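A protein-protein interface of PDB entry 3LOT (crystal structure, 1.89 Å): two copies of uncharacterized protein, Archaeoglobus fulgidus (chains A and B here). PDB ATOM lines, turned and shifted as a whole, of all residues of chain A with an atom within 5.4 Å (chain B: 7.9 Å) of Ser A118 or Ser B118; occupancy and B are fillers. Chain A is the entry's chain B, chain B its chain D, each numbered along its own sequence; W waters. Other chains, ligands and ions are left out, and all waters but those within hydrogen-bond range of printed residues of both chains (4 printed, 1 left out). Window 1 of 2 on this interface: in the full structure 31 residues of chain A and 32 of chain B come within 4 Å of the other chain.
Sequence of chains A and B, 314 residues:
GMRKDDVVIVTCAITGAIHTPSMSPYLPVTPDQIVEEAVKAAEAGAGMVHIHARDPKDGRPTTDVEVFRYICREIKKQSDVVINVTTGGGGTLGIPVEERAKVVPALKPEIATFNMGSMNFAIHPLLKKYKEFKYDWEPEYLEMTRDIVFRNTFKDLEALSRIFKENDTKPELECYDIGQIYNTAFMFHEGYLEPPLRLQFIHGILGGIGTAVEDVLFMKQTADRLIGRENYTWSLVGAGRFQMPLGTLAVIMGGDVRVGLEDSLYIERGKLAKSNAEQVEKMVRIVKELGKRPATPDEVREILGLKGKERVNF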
ATOM      1  N   MET A 116       6.793 -12.464  -1.066  1.00  0.00           N
ATOM      2  CA  MET A 116       5.731 -12.365  -2.072  1.00  0.00           C
ATOM      3  C   MET A 116       5.839 -11.172  -3.053  1.00  0.00           C
ATOM      4  O   MET A 116       4.917 -10.921  -3.790  1.00  0.00           O
ATOM      5  CB  MET A 116       4.370 -12.383  -1.394  1.00  0.00           C
ATOM      6  CG  MET A 116       3.925 -13.802  -0.976  1.00  0.00           C
ATOM      7  SD  MET A 116       3.842 -15.039  -2.400  1.00  0.00           S
ATOM      8  CE  MET A 116       3.068 -13.877  -3.758  1.00  0.00           C
ATOM      9  N   GLY A 117       6.974 -10.492  -3.106  1.00  0.00           N
ATOM     10  CA  GLY A 117       7.176  -9.554  -4.172  1.00  0.00           C
ATOM     11  C   GLY A 117       8.561  -8.929  -4.166  1.00  0.00           C
ATOM     12  O   GLY A 117       9.340  -9.130  -3.220  1.00  0.00           O
ATOM     13  N   SER A 118       8.876  -8.214  -5.239  1.00  0.00           N
ATOM     14  CA  SER A 118      10.135  -7.484  -5.362  1.00  0.00           C
ATOM     15  C   SER A 118       9.913  -6.109  -4.782  1.00  0.00           C
ATOM     16  O   SER A 118       8.833  -5.520  -4.950  1.00  0.00           O
ATOM     17  CB  SER A 118      10.573  -7.343  -6.815  1.00  0.00           C
ATOM     18  OG  SER A 118      10.845  -8.570  -7.433  1.00  0.00           O
ATOM     19  N   MET A 119      10.911  -5.573  -4.090  1.00  0.00           N
ATOM     20  CA  MET A 119      10.749  -4.333  -3.377  1.00  0.00           C
ATOM     21  C   MET A 119      12.094  -3.747  -3.019  1.00  0.00           C
ATOM     22  O   MET A 119      13.101  -4.449  -2.917  1.00  0.00           O
ATOM     23  CB  MET A 119       9.965  -4.532  -2.072  1.00  0.00           C
ATOM     24  CG  MET A 119      10.629  -5.562  -1.110  1.00  0.00           C
ATOM     25  SD  MET A 119       9.646  -6.139   0.452  1.00  0.00           S
ATOM     26  CE  MET A 119       9.672  -4.489   1.468  1.00  0.00           C
ATOM     27  N   ASN A 120      12.076  -2.449  -2.770  1.00  0.00           N
ATOM     28  CA  ASN A 120      13.183  -1.781  -2.061  1.00  0.00           C
ATOM     29  C   ASN A 120      13.137  -2.319  -0.636  1.00  0.00           C
ATOM     30  O   ASN A 120      12.047  -2.596  -0.105  1.00  0.00           O
ATOM     31  CB  ASN A 120      12.981  -0.274  -2.044  1.00  0.00           C
ATOM     32  CG  ASN A 120      13.180   0.375  -3.418  1.00  0.00           C
ATOM     33  OD1 ASN A 120      12.788   1.539  -3.644  1.00  0.00           O
ATOM     34  ND2 ASN A 120      13.788  -0.348  -4.322  1.00  0.00           N
ATOM     35  N   VAL A 149      17.698  -4.217  -4.770  1.00  0.00           N
ATOM     36  CA  VAL A 149      16.330  -4.712  -4.830  1.00  0.00           C
ATOM     37  C   VAL A 149      16.227  -6.086  -4.161  1.00  0.00           C
ATOM     38  O   VAL A 149      16.999  -6.996  -4.460  1.00  0.00           O
ATOM     39  CB  VAL A 149      15.810  -4.779  -6.287  1.00  0.00           C
ATOM     40  CG1 VAL A 149      14.429  -5.462  -6.332  1.00  0.00           C
ATOM     41  CG2 VAL A 149      15.789  -3.358  -6.917  1.00  0.00           C
ATOM     42  N   PHE A 150      15.290  -6.221  -3.242  1.00  0.00           N
ATOM     43  CA  PHE A 150      14.973  -7.523  -2.675  1.00  0.00           C
ATOM     44  C   PHE A 150      14.100  -8.185  -3.727  1.00  0.00           C
ATOM     45  O   PHE A 150      12.913  -7.868  -3.863  1.00  0.00           O
ATOM     46  CB  PHE A 150      14.251  -7.363  -1.332  1.00  0.00           C
ATOM     47  CG  PHE A 150      13.813  -8.665  -0.665  1.00  0.00           C
ATOM     48  CD1 PHE A 150      14.570  -9.823  -0.756  1.00  0.00           C
ATOM     49  CD2 PHE A 150      12.678  -8.686   0.138  1.00  0.00           C
ATOM     50  CE1 PHE A 150      14.138 -11.013  -0.105  1.00  0.00           C
ATOM     51  CE2 PHE A 150      12.247  -9.858   0.801  1.00  0.00           C
ATOM     52  CZ  PHE A 150      13.002 -11.020   0.669  1.00  0.00           C
ATOM     53  N   ARG A 151      14.709  -9.056  -4.511  1.00  0.00           N
ATOM     54  CA  ARG A 151      14.097  -9.526  -5.751  1.00  0.00           C
ATOM     55  C   ARG A 151      13.269 -10.806  -5.585  1.00  0.00           C
ATOM     56  O   ARG A 151      13.770 -11.835  -5.138  1.00  0.00           O
ATOM     57  CB  ARG A 151      15.220  -9.746  -6.780  1.00  0.00           C
ATOM     58  CG  ARG A 151      14.731 -10.172  -8.159  1.00  0.00           C
ATOM     59  CD  ARG A 151      15.911 -10.647  -9.019  1.00  0.00           C
ATOM     60  NE  ARG A 151      15.407 -11.072 -10.307  1.00  0.00           N
ATOM     61  CZ  ARG A 151      15.229 -10.247 -11.337  1.00  0.00           C
ATOM     62  NH1 ARG A 151      15.521  -8.936 -11.224  1.00  0.00           N
ATOM     63  NH2 ARG A 151      14.737 -10.730 -12.473  1.00  0.00           N
ATOM     64  N   ASN A 152      11.992 -10.756  -5.923  1.00  0.00           N
ATOM     65  CA  ASN A 152      11.135 -11.952  -5.900  1.00  0.00           C
ATOM     66  C   ASN A 152      10.068 -11.836  -7.002  1.00  0.00           C
ATOM     67  O   ASN A 152       8.907 -11.460  -6.753  1.00  0.00           O
ATOM     68  CB  ASN A 152      10.473 -12.161  -4.530  1.00  0.00           C
ATOM     69  CG  ASN A 152      11.443 -12.065  -3.366  1.00  0.00           C
ATOM     70  OD1 ASN A 152      12.076 -13.076  -2.991  1.00  0.00           O
ATOM     71  ND2 ASN A 152      11.540 -10.855  -2.744  1.00  0.00           N
ATOM     72  N   THR A 153      10.483 -12.161  -8.229  1.00  0.00           N
ATOM     73  CA  THR A 153       9.651 -11.986  -9.418  1.00  0.00           C
ATOM     74  C   THR A 153       8.595 -13.093  -9.477  1.00  0.00           C
ATOM     75  O   THR A 153       8.725 -14.149  -8.789  1.00  0.00           O
ATOM     76  CB  THR A 153      10.509 -12.040 -10.721  1.00  0.00           C
ATOM     77  OG1 THR A 153      11.019 -13.382 -10.889  1.00  0.00           O
ATOM     78  CG2 THR A 153      11.645 -10.990 -10.734  1.00  0.00           C
ATOM     79  N   GLN A 180       1.447  -7.114  -2.403  1.00  0.00           N
ATOM     80  CA  GLN A 180       1.981  -8.453  -2.237  1.00  0.00           C
ATOM     81  C   GLN A 180       0.891  -9.386  -1.782  1.00  0.00           C
ATOM     82  O   GLN A 180       0.969 -10.539  -2.054  1.00  0.00           O
ATOM     83  CB  GLN A 180       3.156  -8.474  -1.283  1.00  0.00           C
ATOM     84  CG  GLN A 180       4.322  -7.645  -1.855  1.00  0.00           C
ATOM     85  CD  GLN A 180       5.563  -7.697  -1.017  1.00  0.00           C
ATOM     86  OE1 GLN A 180       5.624  -8.405  -0.014  1.00  0.00           O
ATOM     87  NE2 GLN A 180       6.563  -6.940  -1.413  1.00  0.00           N
ATOM     88  N   ASN B 115       8.599   7.323 -10.892  1.00  0.00           N
ATOM     89  CA  ASN B 115       8.133   6.083 -10.238  1.00  0.00           C
ATOM     90  C   ASN B 115       8.786   5.756  -8.870  1.00  0.00           C
ATOM     91  O   ASN B 115      10.023   5.770  -8.723  1.00  0.00           O
ATOM     92  CB  ASN B 115       8.351   4.977 -11.205  1.00  0.00           C
ATOM     93  CG  ASN B 115       7.551   5.197 -12.464  1.00  0.00           C
ATOM     94  OD1 ASN B 115       6.339   4.907 -12.487  1.00  0.00           O
ATOM     95  ND2 ASN B 115       8.207   5.736 -13.526  1.00  0.00           N
ATOM     96  N   MET B 116       7.952   5.499  -7.875  1.00  0.00           N
ATOM     97  CA  MET B 116       8.406   5.587  -6.465  1.00  0.00           C
ATOM     98  C   MET B 116       8.747   4.282  -5.756  1.00  0.00           C
ATOM     99  O   MET B 116       8.845   4.266  -4.527  1.00  0.00           O
ATOM    100  CB  MET B 116       7.344   6.331  -5.665  1.00  0.00           C
ATOM    101  CG  MET B 116       7.261   7.747  -5.986  1.00  0.00           C
ATOM    102  SD  MET B 116       8.875   8.681  -5.456  1.00  0.00           S
ATOM    103  CE  MET B 116       9.131   8.017  -3.698  1.00  0.00           C
ATOM    104  N   GLY B 117       8.983   3.207  -6.491  1.00  0.00           N
ATOM    105  CA  GLY B 117       9.565   2.008  -5.868  1.00  0.00           C
ATOM    106  C   GLY B 117       9.868   0.900  -6.841  1.00  0.00           C
ATOM    107  O   GLY B 117       9.371   0.926  -7.962  1.00  0.00           O
ATOM    108  N   SER B 118      10.686  -0.069  -6.419  1.00  0.00           N
ATOM    109  CA  SER B 118      10.970  -1.243  -7.216  1.00  0.00           C
ATOM    110  C   SER B 118       9.787  -2.199  -7.061  1.00  0.00           C
ATOM    111  O   SER B 118       9.198  -2.303  -5.985  1.00  0.00           O
ATOM    112  CB  SER B 118      12.255  -1.919  -6.774  1.00  0.00           C
ATOM    113  OG  SER B 118      13.325  -1.070  -6.971  1.00  0.00           O
ATOM    114  N   MET B 119       9.399  -2.884  -8.135  1.00  0.00           N
ATOM    115  CA  MET B 119       8.211  -3.751  -8.042  1.00  0.00           C
ATOM    116  C   MET B 119       8.228  -4.765  -9.166  1.00  0.00           C
ATOM    117  O   MET B 119       8.830  -4.530 -10.196  1.00  0.00           O
ATOM    118  CB  MET B 119       6.922  -2.888  -8.136  1.00  0.00           C
ATOM    119  CG  MET B 119       6.727  -2.190  -9.457  1.00  0.00           C
ATOM    120  SD  MET B 119       5.309  -0.868  -9.536  1.00  0.00           S
ATOM    121  CE  MET B 119       3.778  -2.085  -9.538  1.00  0.00           C
ATOM    122  N   ASN B 120       7.488  -5.856  -8.997  1.00  0.00           N
ATOM    123  CA  ASN B 120       7.078  -6.671 -10.146  1.00  0.00           C
ATOM    124  C   ASN B 120       6.109  -5.822 -10.926  1.00  0.00           C
ATOM    125  O   ASN B 120       5.413  -4.988 -10.369  1.00  0.00           O
ATOM    126  CB  ASN B 120       6.428  -7.978  -9.708  1.00  0.00           C
ATOM    127  CG  ASN B 120       7.394  -8.884  -8.949  1.00  0.00           C
ATOM    128  OD1 ASN B 120       8.613  -8.718  -9.036  1.00  0.00           O
ATOM    129  ND2 ASN B 120       6.860  -9.869  -8.248  1.00  0.00           N
ATOM    130  N   PHE B 121       6.093  -6.021 -12.221  1.00  0.00           N
ATOM    131  CA  PHE B 121       5.213  -5.313 -13.113  1.00  0.00           C
ATOM    132  C   PHE B 121       5.018  -6.237 -14.290  1.00  0.00           C
ATOM    133  O   PHE B 121       5.793  -6.210 -15.205  1.00  0.00           O
ATOM    134  CB  PHE B 121       5.835  -3.979 -13.527  1.00  0.00           C
ATOM    135  CG  PHE B 121       4.858  -3.038 -14.176  1.00  0.00           C
ATOM    136  CD1 PHE B 121       4.012  -3.472 -15.204  1.00  0.00           C
ATOM    137  CD2 PHE B 121       4.798  -1.712 -13.787  1.00  0.00           C
ATOM    138  CE1 PHE B 121       3.128  -2.575 -15.813  1.00  0.00           C
ATOM    139  CE2 PHE B 121       3.910  -0.836 -14.391  1.00  0.00           C
ATOM    140  CZ  PHE B 121       3.091  -1.264 -15.391  1.00  0.00           C
ATOM    141  N   ASP B 147       9.628 -11.988 -15.436  1.00  0.00           N
ATOM    142  CA  ASP B 147      10.847 -11.999 -14.649  1.00  0.00           C
ATOM    143  C   ASP B 147      11.663 -10.712 -14.765  1.00  0.00           C
ATOM    144  O   ASP B 147      12.920 -10.753 -14.711  1.00  0.00           O
ATOM    145  CB  ASP B 147      11.672 -13.183 -15.095  1.00  0.00           C
ATOM    146  CG  ASP B 147      12.889 -13.459 -14.194  1.00  0.00           C
ATOM    147  OD1 ASP B 147      12.832 -13.401 -12.934  1.00  0.00           O
ATOM    148  OD2 ASP B 147      13.900 -13.825 -14.795  1.00  0.00           O
ATOM    149  N   ILE B 148      10.990  -9.580 -14.960  1.00  0.00           N
ATOM    150  CA  ILE B 148      11.708  -8.309 -14.984  1.00  0.00           C
ATOM    151  C   ILE B 148      11.217  -7.414 -13.844  1.00  0.00           C
ATOM    152  O   ILE B 148      10.039  -7.171 -13.719  1.00  0.00           O
ATOM    153  CB  ILE B 148      11.627  -7.612 -16.365  1.00  0.00           C
ATOM    154  CG1 ILE B 148      12.621  -8.285 -17.304  1.00  0.00           C
ATOM    155  CG2 ILE B 148      11.995  -6.150 -16.276  1.00  0.00           C
ATOM    156  CD1 ILE B 148      12.456  -7.989 -18.790  1.00  0.00           C
ATOM    157  N   VAL B 149      12.140  -6.940 -13.017  1.00  0.00           N
ATOM    158  CA  VAL B 149      11.786  -5.984 -11.986  1.00  0.00           C
ATOM    159  C   VAL B 149      11.736  -4.584 -12.582  1.00  0.00           C
ATOM    160  O   VAL B 149      12.654  -4.154 -13.285  1.00  0.00           O
ATOM    161  CB  VAL B 149      12.779  -6.075 -10.805  1.00  0.00           C
ATOM    162  CG1 VAL B 149      12.658  -4.844  -9.879  1.00  0.00           C
ATOM    163  CG2 VAL B 149      12.522  -7.396 -10.010  1.00  0.00           C
ATOM    164  N   PHE B 150      10.665  -3.862 -12.288  1.00  0.00           N
ATOM    165  CA  PHE B 150      10.608  -2.425 -12.585  1.00  0.00           C
ATOM    166  C   PHE B 150      11.314  -1.734 -11.446  1.00  0.00           C
ATOM    167  O   PHE B 150      10.756  -1.602 -10.351  1.00  0.00           O
ATOM    168  CB  PHE B 150       9.156  -1.990 -12.654  1.00  0.00           C
ATOM    169  CG  PHE B 150       8.943  -0.579 -13.003  1.00  0.00           C
ATOM    170  CD1 PHE B 150       9.742   0.075 -13.932  1.00  0.00           C
ATOM    171  CD2 PHE B 150       7.878   0.115 -12.433  1.00  0.00           C
ATOM    172  CE1 PHE B 150       9.516   1.429 -14.247  1.00  0.00           C
ATOM    173  CE2 PHE B 150       7.619   1.455 -12.742  1.00  0.00           C
ATOM    174  CZ  PHE B 150       8.450   2.122 -13.648  1.00  0.00           C
ATOM    175  N   ARG B 151      12.534  -1.296 -11.705  1.00  0.00           N
ATOM    176  CA  ARG B 151      13.485  -0.971 -10.658  1.00  0.00           C
ATOM    177  C   ARG B 151      13.569   0.543 -10.367  1.00  0.00           C
ATOM    178  O   ARG B 151      13.819   1.350 -11.274  1.00  0.00           O
ATOM    179  CB  ARG B 151      14.856  -1.499 -11.090  1.00  0.00           C
ATOM    180  CG  ARG B 151      15.990  -1.304 -10.065  1.00  0.00           C
ATOM    181  CD  ARG B 151      17.353  -1.267 -10.717  1.00  0.00           C
ATOM    182  NE  ARG B 151      18.378  -1.125  -9.683  1.00  0.00           N
ATOM    183  CZ  ARG B 151      18.852  -2.137  -8.962  1.00  0.00           C
ATOM    184  NH1 ARG B 151      18.414  -3.385  -9.169  1.00  0.00           N
ATOM    185  NH2 ARG B 151      19.788  -1.907  -8.047  1.00  0.00           N
ATOM    186  N   ASN B 152      13.381   0.926  -9.104  1.00  0.00           N
ATOM    187  CA  ASN B 152      13.505   2.323  -8.709  1.00  0.00           C
ATOM    188  C   ASN B 152      13.942   2.341  -7.246  1.00  0.00           C
ATOM    189  O   ASN B 152      13.115   2.470  -6.347  1.00  0.00           O
ATOM    190  CB  ASN B 152      12.188   3.101  -8.918  1.00  0.00           C
ATOM    191  CG  ASN B 152      11.601   2.933 -10.343  1.00  0.00           C
ATOM    192  OD1 ASN B 152      11.938   3.722 -11.246  1.00  0.00           O
ATOM    193  ND2 ASN B 152      10.678   1.926 -10.541  1.00  0.00           N
ATOM    194  N   THR B 153      15.230   2.148  -7.030  1.00  0.00           N
ATOM    195  CA  THR B 153      15.785   2.052  -5.702  1.00  0.00           C
ATOM    196  C   THR B 153      15.895   3.430  -5.043  1.00  0.00           C
ATOM    197  O   THR B 153      15.753   4.435  -5.709  1.00  0.00           O
ATOM    198  CB  THR B 153      17.209   1.457  -5.714  1.00  0.00           C
ATOM    199  OG1 THR B 153      18.111   2.378  -6.320  1.00  0.00           O
ATOM    200  CG2 THR B 153      17.265   0.083  -6.439  1.00  0.00           C
ATOM    201  N   PHE B 154      16.118   3.468  -3.740  1.00  0.00           N
ATOM    202  CA  PHE B 154      16.242   4.732  -3.064  1.00  0.00           C
ATOM    203  C   PHE B 154      17.435   5.497  -3.608  1.00  0.00           C
ATOM    204  O   PHE B 154      17.360   6.701  -3.844  1.00  0.00           O
ATOM    205  CB  PHE B 154      16.306   4.543  -1.550  1.00  0.00           C
ATOM    206  CG  PHE B 154      14.980   4.220  -0.952  1.00  0.00           C
ATOM    207  CD1 PHE B 154      14.014   5.187  -0.834  1.00  0.00           C
ATOM    208  CD2 PHE B 154      14.687   2.933  -0.515  1.00  0.00           C
ATOM    209  CE1 PHE B 154      12.779   4.898  -0.282  1.00  0.00           C
ATOM    210  CE2 PHE B 154      13.451   2.635   0.021  1.00  0.00           C
ATOM    211  CZ  PHE B 154      12.480   3.631   0.119  1.00  0.00           C
ATOM    212  N   ASP B 156      18.502   5.261  -6.735  1.00  0.00           N
ATOM    213  CA  ASP B 156      17.981   5.779  -8.016  1.00  0.00           C
ATOM    214  C   ASP B 156      17.141   7.055  -7.781  1.00  0.00           C
ATOM    215  O   ASP B 156      17.280   8.034  -8.497  1.00  0.00           O
ATOM    216  CB  ASP B 156      17.049   4.775  -8.691  1.00  0.00           C
ATOM    217  CG  ASP B 156      17.761   3.529  -9.233  1.00  0.00           C
ATOM    218  OD1 ASP B 156      18.981   3.553  -9.482  1.00  0.00           O
ATOM    219  OD2 ASP B 156      17.039   2.527  -9.439  1.00  0.00           O
ATOM    220  N   LEU B 157      16.262   7.020  -6.785  1.00  0.00           N
ATOM    221  CA  LEU B 157      15.322   8.127  -6.556  1.00  0.00           C
ATOM    222  C   LEU B 157      16.035   9.401  -6.065  1.00  0.00           C
ATOM    223  O   LEU B 157      15.629  10.522  -6.396  1.00  0.00           O
ATOM    224  CB  LEU B 157      14.214   7.712  -5.573  1.00  0.00           C
ATOM    225  CG  LEU B 157      13.402   6.498  -6.039  1.00  0.00           C
ATOM    226  CD1 LEU B 157      12.450   6.027  -4.952  1.00  0.00           C
ATOM    227  CD2 LEU B 157      12.678   6.807  -7.353  1.00  0.00           C
ATOM    228  N   ASP B 177       1.340   1.366  -4.943  1.00  0.00           N
ATOM    229  CA  ASP B 177       1.064   0.614  -3.718  1.00  0.00           C
ATOM    230  C   ASP B 177       1.235   1.555  -2.504  1.00  0.00           C
ATOM    231  O   ASP B 177       1.814   2.644  -2.607  1.00  0.00           O
ATOM    232  CB  ASP B 177       2.058  -0.550  -3.588  1.00  0.00           C
ATOM    233  CG  ASP B 177       1.461  -1.795  -2.984  1.00  0.00           C
ATOM    234  OD1 ASP B 177       0.450  -1.757  -2.224  1.00  0.00           O
ATOM    235  OD2 ASP B 177       2.052  -2.865  -3.273  1.00  0.00           O
ATOM    236  N   GLN B 180       4.767   2.555  -1.494  1.00  0.00           N
ATOM    237  CA  GLN B 180       5.321   3.611  -2.361  1.00  0.00           C
ATOM    238  C   GLN B 180       4.891   5.026  -1.943  1.00  0.00           C
ATOM    239  O   GLN B 180       5.617   6.016  -2.168  1.00  0.00           O
ATOM    240  CB  GLN B 180       4.939   3.334  -3.829  1.00  0.00           C
ATOM    241  CG  GLN B 180       5.558   2.013  -4.351  1.00  0.00           C
ATOM    242  CD  GLN B 180       5.500   1.844  -5.857  1.00  0.00           C
ATOM    243  OE1 GLN B 180       4.987   2.695  -6.591  1.00  0.00           O
ATOM    244  NE2 GLN B 180       6.027   0.723  -6.330  1.00  0.00           N
ATOM    245  N   ASN B 183       7.284   5.373   0.743  1.00  0.00           N
ATOM    246  CA  ASN B 183       8.549   5.777   0.118  1.00  0.00           C
ATOM    247  C   ASN B 183       8.531   7.295  -0.203  1.00  0.00           C
ATOM    248  O   ASN B 183       9.525   8.013   0.049  1.00  0.00           O
ATOM    249  CB  ASN B 183       8.869   4.993  -1.159  1.00  0.00           C
ATOM    250  CG  ASN B 183       9.105   3.481  -0.937  1.00  0.00           C
ATOM    251  OD1 ASN B 183       9.152   2.985   0.203  1.00  0.00           O
ATOM    252  ND2 ASN B 183       9.215   2.729  -2.070  1.00  0.00           N
ATOM    253  N   GLY B 207       1.424  -6.788  -9.614  1.00  0.00           N
ATOM    254  CA  GLY B 207       2.637  -6.342  -8.948  1.00  0.00           C
ATOM    255  C   GLY B 207       2.376  -5.135  -8.075  1.00  0.00           C
ATOM    256  O   GLY B 207       3.215  -4.757  -7.244  1.00  0.00           O
HETATM  257  O   HOH W   1      14.609 -13.695 -11.177  1.00  0.00           O
HETATM  258  O   HOH W   2      15.049  -7.396 -13.917  1.00  0.00           O
HETATM  259  O   HOH W   3      19.827  -5.016  -6.956  1.00  0.00           O
HETATM  260  O   HOH W   4       6.467  -6.668  -6.463  1.00  0.00           O
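Among the printed residues, pairs that only touch across the chains: Ser A118 with Met B119 (3.6 Å), Ser A118 with Val B149 (3.3 Å), Met A119 with Ser B118 (3.7 Å), Asn A120 with Gly B117 (3.9 Å), Asn A120 with Thr B153 (3.4 Å), Asn A120 with Phe B154 (3.6 Å), Val A149 with Ser B118 (3.4 Å), Val A149 with Arg B151 (3.5 Å), Val A149 with Thr B153 (3.8 Å), Arg A151 with Val B149 (3.6 Å), Thr A153 with Asn B120 (3.5 Å) and Thr A153 with Val B149 (3.8 Å).
The backbone carbonyl oxygen (O) of Gly A117 lies within hydrogen-bond range of the side-chain amide nitrogen (ND2) of Asn A152, at 2.8 Å. The backbone NH (N) of Phe A150 sits at hydrogen-bond distance from the backbone carbonyl oxygen (O) of Met A119, 2.8 Å away. The side-chain amide nitrogen of Asn B152 lies within hydrogen-bond range of the backbone carbonyl oxygen of Gly B117, at 3.1 Å. The backbone carbonyl oxygen (O) of Met B119 lies within hydrogen-bond range of the backbone NH (N) of Phe B150 (2.9 Å). NE of Arg B151 is in salt-bridge range of OD2 of Asp B156. OG1 of Thr B153 lies within hydrogen-bond range of N of Asp B156 (2.9 Å).
Printed residues of chain B within 4 Å of Ser A118: Ser B118, Met B119, Asn B120 and Val B149. Of the printed residues of chain B, Met A119 touches Ser B118 (3.7 Å). Phe A150 touches none of the printed residues of chain B. Ser B118 touches just these residues of chain A: Ser A118 (3.4 Å), Met A119 (3.7 Å), Asn A120 (2.8 Å) and Val A149 (3.4 Å). Of the printed residues of chain A, Val B149 touches Ser A118 (3.3 Å), Arg A151 (3.6 Å) and Thr A153 (3.8 Å). Of the printed residues of chain A, Asn B152 touches Asn A120. The nearest residue of chain B that does not touch Ser A118 is Gly B207 (6.1 Å). The nearest printed residue of chain A that does not touch Ser B118 is Phe A150 (6.3 Å).
Water W1 lies within hydrogen-bond range of the side-chain carboxylate (OD1) of Asp B147 and the guanidinium group (NE) of Arg A151. Water W4 lies within hydrogen-bond range of the backbone NH of Asn B120 (2.9 Å) and the backbone carbonyl oxygen of Ser A118 (3.0 Å). Water W2 lies within hydrogen-bond range of the backbone NH of Val B149 (3.1 Å) and the guanidinium group of Arg A151 (3.1 Å). Water W3 bridges NH1 of Arg B151 (3.1 Å) and N of Val A149 (3.2 Å).
The side-chain amide oxygen (OD1) of Asn B120 is in hydrogen-bond range of the side-chain hydroxyl (OG) of Ser A118. The side-chain amide nitrogen (ND2) of Asn A120 lies within hydrogen-bond range of the side-chain hydroxyl (OG) of Ser B118, at 2.8 Å. O of Asn B152 lies close to OD1 of Asn A120 (2.9 Å). The guanidinium group of Arg A151 lies within salt-bridge range of the side-chain carboxylate of Asp B147. The backbone carbonyl oxygen (O) of Asn A152 sits at hydrogen-bond distance from the side-chain amide nitrogen (ND2) of Asn B120, at 3.0 Å. The side-chain hydroxyl (OG1) of Thr A153 sits at hydrogen-bond distance from the side-chain carboxylate (OD1) of Asp B147 (2.7 Å). O of Ser A118 sits close to O of Ser B118, at 3.4 Å.
Ser A118 touches its own counterpart, Ser B118. Asn A120 touches Gly B117, but with the chains exchanged Gly A117 does not touch Asn B120 (4.1 Å). Asn A120 touches Asn B152, and with the chains exchanged Asn A152 touches Asn B120. Val A149 touches Thr B153, and with the chains exchanged Thr A153 touches Val B149. Positions printed for both chains: 116, 117, 118, 119, 120, 149, 150, 151, 152, 153 and 180. Of the 19 pairs that touch across the chains among the printed residues, 15 have their exchanged pair printed and touching as well.
Of the 11 printed residues of chain A, 7 touch a printed residue of chain B. Printed residues of chain A that touch a printed residue of chain B: Ser A118, Met A119, Asn A120, Val A149, Arg A151, Asn A152 and Thr A153. Hydrophobic or aromatic side chains of chain A within 4 Å of the printed part of chain B: Val A149. Among the printed residues, 19 pairs touch across the chains. Among the printed residues, Asp or Glu carboxylates within 4 Å of a Lys or Arg side-chain nitrogen of the other chain: Arg A151 with Asp B147.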
